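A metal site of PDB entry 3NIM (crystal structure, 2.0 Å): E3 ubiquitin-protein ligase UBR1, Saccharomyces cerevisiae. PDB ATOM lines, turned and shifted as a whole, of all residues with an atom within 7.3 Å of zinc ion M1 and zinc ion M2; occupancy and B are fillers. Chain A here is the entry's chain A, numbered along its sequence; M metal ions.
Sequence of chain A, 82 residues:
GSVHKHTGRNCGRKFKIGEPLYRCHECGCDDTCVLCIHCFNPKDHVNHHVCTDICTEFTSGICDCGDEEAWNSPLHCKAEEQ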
ATOM      1  N   HIS A   4      29.732   8.755  -3.793  1.00  0.00           N
ATOM      2  CA  HIS A   4      31.171   8.567  -3.784  1.00  0.00           C
ATOM      3  C   HIS A   4      31.364   7.413  -2.834  1.00  0.00           C
ATOM      4  O   HIS A   4      31.180   7.541  -1.630  1.00  0.00           O
ATOM      5  CB  HIS A   4      31.916   9.812  -3.273  1.00  0.00           C
ATOM      6  CG  HIS A   4      31.206  11.115  -3.536  1.00  0.00           C
ATOM      7  ND1 HIS A   4      30.537  11.820  -2.548  1.00  0.00           N
ATOM      8  CD2 HIS A   4      31.088  11.855  -4.667  1.00  0.00           C
ATOM      9  CE1 HIS A   4      30.033  12.927  -3.058  1.00  0.00           C
ATOM     10  NE2 HIS A   4      30.347  12.973  -4.344  1.00  0.00           N
ATOM     11  N   LYS A   5      31.676   6.251  -3.399  1.00  0.00           N
ATOM     12  CA  LYS A   5      31.806   5.023  -2.640  1.00  0.00           C
ATOM     13  C   LYS A   5      33.158   5.037  -1.933  1.00  0.00           C
ATOM     14  O   LYS A   5      34.064   5.755  -2.341  1.00  0.00           O
ATOM     15  CB  LYS A   5      31.721   3.795  -3.569  1.00  0.00           C
ATOM     16  CG  LYS A   5      30.476   3.739  -4.480  1.00  0.00           C
ATOM     17  CD  LYS A   5      30.634   2.669  -5.561  1.00  0.00           C
ATOM     18  CE  LYS A   5      29.368   2.533  -6.448  1.00  0.00           C
ATOM     19  NZ  LYS A   5      29.087   3.766  -7.244  1.00  0.00           N
ATOM     20  N   HIS A   6      33.273   4.246  -0.869  1.00  0.00           N
ATOM     21  CA  HIS A   6      34.546   4.065  -0.161  1.00  0.00           C
ATOM     22  C   HIS A   6      34.911   2.566  -0.100  1.00  0.00           C
ATOM     23  O   HIS A   6      35.342   2.060   0.937  1.00  0.00           O
ATOM     24  CB  HIS A   6      34.447   4.675   1.247  1.00  0.00           C
ATOM     25  CG  HIS A   6      33.373   4.073   2.100  1.00  0.00           C
ATOM     26  ND1 HIS A   6      33.574   2.902   2.804  1.00  0.00           N
ATOM     27  CD2 HIS A   6      32.096   4.451   2.342  1.00  0.00           C
ATOM     28  CE1 HIS A   6      32.462   2.602   3.453  1.00  0.00           C
ATOM     29  NE2 HIS A   6      31.548   3.515   3.178  1.00  0.00           N
ATOM     30  N   ARG A   9      37.586   0.151   2.002  1.00  0.00           N
ATOM     31  CA  ARG A   9      38.022   0.941   3.163  1.00  0.00           C
ATOM     32  C   ARG A   9      36.845   1.527   3.962  1.00  0.00           C
ATOM     33  O   ARG A   9      35.707   1.435   3.539  1.00  0.00           O
ATOM     34  CB  ARG A   9      38.977   2.068   2.732  1.00  0.00           C
ATOM     35  CG  ARG A   9      38.470   2.903   1.571  1.00  0.00           C
ATOM     36  CD  ARG A   9      39.031   4.308   1.589  1.00  0.00           C
ATOM     37  NE  ARG A   9      38.461   5.085   2.682  1.00  0.00           N
ATOM     38  CZ  ARG A   9      38.770   6.344   2.947  1.00  0.00           C
ATOM     39  NH1 ARG A   9      39.668   6.990   2.228  1.00  0.00           N
ATOM     40  NH2 ARG A   9      38.175   6.959   3.954  1.00  0.00           N
ATOM     41  N   ASN A  10      37.154   2.156   5.084  1.00  0.00           N
ATOM     42  CA  ASN A  10      36.127   2.792   5.906  1.00  0.00           C
ATOM     43  C   ASN A  10      35.650   4.068   5.257  1.00  0.00           C
ATOM     44  O   ASN A  10      36.323   4.615   4.378  1.00  0.00           O
ATOM     45  CB  ASN A  10      36.665   3.117   7.294  1.00  0.00           C
ATOM     46  CG  ASN A  10      37.747   4.182   7.234  1.00  0.00           C
ATOM     47  OD1 ASN A  10      38.653   4.088   6.410  1.00  0.00           O
ATOM     48  ND2 ASN A  10      37.629   5.210   8.059  1.00  0.00           N
ATOM     49  N   CYS A  11      34.484   4.531   5.685  1.00  0.00           N
ATOM     50  CA  CYS A  11      33.987   5.838   5.307  1.00  0.00           C
ATOM     51  C   CYS A  11      34.831   6.967   5.903  1.00  0.00           C
ATOM     52  O   CYS A  11      35.497   7.700   5.168  1.00  0.00           O
ATOM     53  CB  CYS A  11      32.541   5.990   5.723  1.00  0.00           C
ATOM     54  SG  CYS A  11      31.873   7.592   5.212  1.00  0.00           S
ATOM     55  N   GLY A  12      34.763   7.124   7.224  1.00  0.00           N
ATOM     56  CA  GLY A  12      35.550   8.153   7.929  1.00  0.00           C
ATOM     57  C   GLY A  12      35.140   9.582   7.644  1.00  0.00           C
ATOM     58  O   GLY A  12      35.861  10.512   8.032  1.00  0.00           O
ATOM     59  N   ARG A  13      34.002   9.776   6.967  1.00  0.00           N
ATOM     60  CA  ARG A  13      33.521  11.121   6.582  1.00  0.00           C
ATOM     61  C   ARG A  13      33.129  11.930   7.813  1.00  0.00           C
ATOM     62  O   ARG A  13      32.434  11.437   8.681  1.00  0.00           O
ATOM     63  CB  ARG A  13      32.352  10.999   5.590  1.00  0.00           C
ATOM     64  CG  ARG A  13      31.624  12.303   5.238  1.00  0.00           C
ATOM     65  CD  ARG A  13      30.406  12.023   4.358  1.00  0.00           C
ATOM     66  NE  ARG A  13      29.743  13.236   3.874  1.00  0.00           N
ATOM     67  CZ  ARG A  13      28.908  13.996   4.589  1.00  0.00           C
ATOM     68  NH1 ARG A  13      28.610  13.699   5.865  1.00  0.00           N
ATOM     69  NH2 ARG A  13      28.351  15.063   4.021  1.00  0.00           N
ATOM     70  N   PHE A  15      30.965  14.480   9.759  1.00  0.00           N
ATOM     71  CA  PHE A  15      29.603  15.020   9.666  1.00  0.00           C
ATOM     72  C   PHE A  15      29.646  16.522   9.460  1.00  0.00           C
ATOM     73  O   PHE A  15      30.508  17.202  10.002  1.00  0.00           O
ATOM     74  CB  PHE A  15      28.785  14.669  10.925  1.00  0.00           C
ATOM     75  CG  PHE A  15      28.618  13.194  11.122  1.00  0.00           C
ATOM     76  CD1 PHE A  15      27.613  12.496  10.468  1.00  0.00           C
ATOM     77  CD2 PHE A  15      29.500  12.485  11.924  1.00  0.00           C
ATOM     78  CE1 PHE A  15      27.482  11.115  10.630  1.00  0.00           C
ATOM     79  CE2 PHE A  15      29.375  11.112  12.095  1.00  0.00           C
ATOM     80  CZ  PHE A  15      28.374  10.423  11.441  1.00  0.00           C
ATOM     81  N   VAL A  34      28.545   5.224  14.713  1.00  0.00           N
ATOM     82  CA  VAL A  34      27.611   6.055  13.934  1.00  0.00           C
ATOM     83  C   VAL A  34      27.808   5.934  12.393  1.00  0.00           C
ATOM     84  O   VAL A  34      28.896   5.565  11.927  1.00  0.00           O
ATOM     85  CB  VAL A  34      27.650   7.556  14.360  1.00  0.00           C
ATOM     86  CG1 VAL A  34      27.066   7.763  15.778  1.00  0.00           C
ATOM     87  CG2 VAL A  34      29.055   8.117  14.275  1.00  0.00           C
ATOM     88  N   LEU A  35      26.741   6.219  11.644  1.00  0.00           N
ATOM     89  CA  LEU A  35      26.794   6.196  10.167  1.00  0.00           C
ATOM     90  C   LEU A  35      26.269   7.502   9.601  1.00  0.00           C
ATOM     91  O   LEU A  35      25.427   8.171  10.214  1.00  0.00           O
ATOM     92  CB  LEU A  35      25.962   5.028   9.606  1.00  0.00           C
ATOM     93  CG  LEU A  35      26.349   3.584   9.975  1.00  0.00           C
ATOM     94  CD1 LEU A  35      25.212   2.576   9.806  1.00  0.00           C
ATOM     95  CD2 LEU A  35      27.603   3.127   9.209  1.00  0.00           C
ATOM     96  N   CYS A  36      26.776   7.885   8.444  1.00  0.00           N
ATOM     97  CA  CYS A  36      26.356   9.132   7.814  1.00  0.00           C
ATOM     98  C   CYS A  36      25.202   8.871   6.825  1.00  0.00           C
ATOM     99  O   CYS A  36      24.840   7.726   6.539  1.00  0.00           O
ATOM    100  CB  CYS A  36      27.537   9.800   7.114  1.00  0.00           C
ATOM    101  SG  CYS A  36      28.026   8.934   5.617  1.00  0.00           S
ATOM    102  N   ILE A  37      24.628   9.955   6.302  1.00  0.00           N
ATOM    103  CA  ILE A  37      23.509   9.918   5.363  1.00  0.00           C
ATOM    104  C   ILE A  37      23.865   9.128   4.078  1.00  0.00           C
ATOM    105  O   ILE A  37      22.977   8.563   3.421  1.00  0.00           O
ATOM    106  CB  ILE A  37      23.087  11.346   4.967  1.00  0.00           C
ATOM    107  CG1 ILE A  37      24.333  12.190   4.623  1.00  0.00           C
ATOM    108  CG2 ILE A  37      22.291  12.006   6.092  1.00  0.00           C
ATOM    109  CD1 ILE A  37      24.089  13.534   3.976  1.00  0.00           C
ATOM    110  N   HIS A  38      25.156   9.101   3.721  1.00  0.00           N
ATOM    111  CA  HIS A  38      25.594   8.436   2.499  1.00  0.00           C
ATOM    112  C   HIS A  38      25.554   6.922   2.693  1.00  0.00           C
ATOM    113  O   HIS A  38      25.353   6.158   1.742  1.00  0.00           O
ATOM    114  CB  HIS A  38      26.998   8.844   2.101  1.00  0.00           C
ATOM    115  CG  HIS A  38      27.155  10.298   1.741  1.00  0.00           C
ATOM    116  ND1 HIS A  38      26.233  11.257   2.083  1.00  0.00           N
ATOM    117  CD2 HIS A  38      28.152  10.950   1.108  1.00  0.00           C
ATOM    118  CE1 HIS A  38      26.644  12.439   1.662  1.00  0.00           C
ATOM    119  NE2 HIS A  38      27.799  12.276   1.057  1.00  0.00           N
ATOM    120  N   CYS A  39      25.751   6.495   3.938  1.00  0.00           N
ATOM    121  CA  CYS A  39      26.110   5.101   4.225  1.00  0.00           C
ATOM    122  C   CYS A  39      24.985   4.290   4.809  1.00  0.00           C
ATOM    123  O   CYS A  39      24.853   3.093   4.502  1.00  0.00           O
ATOM    124  CB  CYS A  39      27.315   5.075   5.174  1.00  0.00           C
ATOM    125  SG  CYS A  39      28.880   5.447   4.340  1.00  0.00           S
ATOM    126  N   PHE A  40      24.217   4.924   5.692  1.00  0.00           N
ATOM    127  CA  PHE A  40      23.120   4.282   6.413  1.00  0.00           C
ATOM    128  C   PHE A  40      22.159   3.666   5.415  1.00  0.00           C
ATOM    129  O   PHE A  40      21.603   4.367   4.582  1.00  0.00           O
ATOM    130  CB  PHE A  40      22.396   5.317   7.273  1.00  0.00           C
ATOM    131  CG  PHE A  40      21.244   4.754   8.041  1.00  0.00           C
ATOM    132  CD1 PHE A  40      21.449   4.114   9.262  1.00  0.00           C
ATOM    133  CD2 PHE A  40      19.945   4.862   7.533  1.00  0.00           C
ATOM    134  CE1 PHE A  40      20.387   3.578   9.968  1.00  0.00           C
ATOM    135  CE2 PHE A  40      18.866   4.324   8.222  1.00  0.00           C
ATOM    136  CZ  PHE A  40      19.076   3.692   9.443  1.00  0.00           C
ATOM    137  N   ILE A  62      33.112  11.185  12.996  1.00  0.00           N
ATOM    138  CA  ILE A  62      33.260  10.638  11.629  1.00  0.00           C
ATOM    139  C   ILE A  62      32.439   9.370  11.504  1.00  0.00           C
ATOM    140  O   ILE A  62      32.165   8.709  12.511  1.00  0.00           O
ATOM    141  CB  ILE A  62      34.720  10.333  11.296  1.00  0.00           C
ATOM    142  CG1 ILE A  62      35.310   9.387  12.350  1.00  0.00           C
ATOM    143  CG2 ILE A  62      35.543  11.629  11.261  1.00  0.00           C
ATOM    144  CD1 ILE A  62      36.030   8.176  11.808  1.00  0.00           C
ATOM    145  N   CYS A  63      32.055   9.046  10.265  1.00  0.00           N
ATOM    146  CA  CYS A  63      31.229   7.885   9.989  1.00  0.00           C
ATOM    147  C   CYS A  63      32.011   6.575  10.128  1.00  0.00           C
ATOM    148  O   CYS A  63      33.119   6.453   9.585  1.00  0.00           O
ATOM    149  CB  CYS A  63      30.637   8.018   8.569  1.00  0.00           C
ATOM    150  SG  CYS A  63      29.814   6.546   8.024  1.00  0.00           S
ATOM    151  N   ASP A  64      31.431   5.582  10.830  1.00  0.00           N
ATOM    152  CA  ASP A  64      32.073   4.280  11.033  1.00  0.00           C
ATOM    153  C   ASP A  64      31.799   3.177   9.995  1.00  0.00           C
ATOM    154  O   ASP A  64      32.258   2.051  10.164  1.00  0.00           O
ATOM    155  CB  ASP A  64      31.790   3.739  12.432  1.00  0.00           C
ATOM    156  CG  ASP A  64      32.260   4.681  13.523  1.00  0.00           C
ATOM    157  OD1 ASP A  64      33.394   5.202  13.465  1.00  0.00           O
ATOM    158  OD2 ASP A  64      31.481   4.910  14.444  1.00  0.00           O
ATOM    159  N   CYS A  65      31.085   3.498   8.920  1.00  0.00           N
ATOM    160  CA  CYS A  65      30.843   2.514   7.881  1.00  0.00           C
ATOM    161  C   CYS A  65      32.152   1.934   7.326  1.00  0.00           C
ATOM    162  O   CYS A  65      33.042   2.679   6.996  1.00  0.00           O
ATOM    163  CB  CYS A  65      30.046   3.174   6.735  1.00  0.00           C
ATOM    164  SG  CYS A  65      29.417   1.989   5.570  1.00  0.00           S
ATOM    165  N   GLY A  66      32.254   0.608   7.244  1.00  0.00           N
ATOM    166  CA  GLY A  66      33.462  -0.036   6.719  1.00  0.00           C
ATOM    167  C   GLY A  66      34.549  -0.309   7.761  1.00  0.00           C
ATOM    168  O   GLY A  66      35.535  -0.991   7.490  1.00  0.00           O
ATOM    169  N   LEU A  75      27.412  -4.653   7.330  1.00  0.00           N
ATOM    170  CA  LEU A  75      26.597  -3.565   6.765  1.00  0.00           C
ATOM    171  C   LEU A  75      26.722  -3.532   5.242  1.00  0.00           C
ATOM    172  O   LEU A  75      27.758  -3.873   4.675  1.00  0.00           O
ATOM    173  CB  LEU A  75      26.994  -2.193   7.314  1.00  0.00           C
ATOM    174  CG  LEU A  75      26.937  -1.870   8.805  1.00  0.00           C
ATOM    175  CD1 LEU A  75      27.410  -0.455   9.032  1.00  0.00           C
ATOM    176  CD2 LEU A  75      25.561  -2.078   9.384  1.00  0.00           C
ATOM    177  N   HIS A  76      25.653  -3.084   4.603  1.00  0.00           N
ATOM    178  CA  HIS A  76      25.623  -2.981   3.153  1.00  0.00           C
ATOM    179  C   HIS A  76      25.477  -1.510   2.862  1.00  0.00           C
ATOM    180  O   HIS A  76      24.380  -0.992   2.745  1.00  0.00           O
ATOM    181  CB  HIS A  76      24.468  -3.811   2.610  1.00  0.00           C
ATOM    182  CG  HIS A  76      24.464  -5.222   3.125  1.00  0.00           C
ATOM    183  ND1 HIS A  76      23.955  -5.551   4.369  1.00  0.00           N
ATOM    184  CD2 HIS A  76      24.948  -6.366   2.595  1.00  0.00           C
ATOM    185  CE1 HIS A  76      24.112  -6.858   4.565  1.00  0.00           C
ATOM    186  NE2 HIS A  76      24.713  -7.363   3.508  1.00  0.00           N
ATOM    187  N   CYS A  77      26.625  -0.840   2.808  1.00  0.00           N
ATOM    188  CA  CYS A  77      26.696   0.592   2.621  1.00  0.00           C
ATOM    189  C   CYS A  77      25.720   1.001   1.547  1.00  0.00           C
ATOM    190  O   CYS A  77      25.709   0.419   0.465  1.00  0.00           O
ATOM    191  CB  CYS A  77      28.127   0.988   2.218  1.00  0.00           C
ATOM    192  SG  CYS A  77      28.345   2.744   1.861  1.00  0.00           S
ATOM    193  N   LYS A  78      24.919   2.028   1.837  1.00  0.00           N
ATOM    194  CA  LYS A  78      23.976   2.606   0.868  1.00  0.00           C
ATOM    195  C   LYS A  78      24.635   3.088  -0.423  1.00  0.00           C
ATOM    196  O   LYS A  78      24.047   2.951  -1.497  1.00  0.00           O
ATOM    197  CB  LYS A  78      23.177   3.750   1.498  1.00  0.00           C
ATOM    198  CG  LYS A  78      21.934   4.120   0.684  1.00  0.00           C
ATOM    199  CD  LYS A  78      21.230   5.345   1.216  1.00  0.00           C
ATOM    200  CE  LYS A  78      19.993   5.636   0.383  1.00  0.00           C
ATOM    201  NZ  LYS A  78      19.038   4.470   0.361  1.00  0.00           N
ATOM    202  N   ALA A  79      25.833   3.650  -0.323  1.00  0.00           N
ATOM    203  CA  ALA A  79      26.553   4.165  -1.498  1.00  0.00           C
ATOM    204  C   ALA A  79      26.875   3.094  -2.544  1.00  0.00           C
ATOM    205  O   ALA A  79      27.046   3.392  -3.729  1.00  0.00           O
ATOM    206  CB  ALA A  79      27.844   4.870  -1.051  1.00  0.00           C
ATOM    207  N   GLU A  80      26.940   1.843  -2.103  1.00  0.00           N
ATOM    208  CA  GLU A  80      27.303   0.701  -2.950  1.00  0.00           C
ATOM    209  C   GLU A  80      26.150   0.191  -3.814  1.00  0.00           C
ATOM    210  O   GLU A  80      26.365  -0.569  -4.768  1.00  0.00           O
ATOM    211  CB  GLU A  80      27.843  -0.436  -2.092  1.00  0.00           C
ATOM    212  CG  GLU A  80      29.174  -0.134  -1.421  1.00  0.00           C
ATOM    213  CD  GLU A  80      30.338  -0.088  -2.392  1.00  0.00           C
ATOM    214  OE1 GLU A  80      30.319  -0.848  -3.390  1.00  0.00           O
ATOM    215  OE2 GLU A  80      31.265   0.706  -2.163  1.00  0.00           O
HETATM  216 ZN    ZN M   1      29.556   3.442   3.726  1.00  0.00          ZN
HETATM  217 ZN    ZN M   2      29.670   7.273   5.826  1.00  0.00          ZN
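Of the 27 residues printed, 4 come within 4 Å of zinc ion M2.
The nearest printed residue that does not touch zinc ion M2 is Cys 65 (4.2 Å).
Zinc ion M2 is bound by SG of Cys 11, SG of Cys 63, SG of Cys 36 and SG of Cys 39.
Zinc ion M1 is bound by NE2 of His 6 (2.1 Å), SG of Cys 39 (2.2 Å), SG of Cys 77 (2.3 Å) and SG of Cys 65 (2.4 Å).
ND1 of His 6 is in hydrogen-bond range of O of Arg 9 (2.7 Å).
The backbone carbonyl oxygen (O) of Cys 39 is in hydrogen-bond range of the backbone NH (N) of Lys 78 (2.9 Å).
O of Cys 65 lies within hydrogen-bond range of N of Cys 11 (2.7 Å).
The side-chain sulfur (SG) of Cys 11 lies close to the backbone NH (N) of Arg 13.
O of Cys 11 lies within hydrogen-bond range of NH2 of Arg 9, at 3.0 Å.
The side-chain sulfur (SG) of Cys 63 lies close to the backbone NH (N) of Cys 65.
The backbone NH (N) of Cys 63 lies within hydrogen-bond range of the backbone carbonyl oxygen (O) of Arg 13 (2.9 Å).
O of Cys 63 lies within hydrogen-bond range of N of Gly 12 (3.0 Å).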
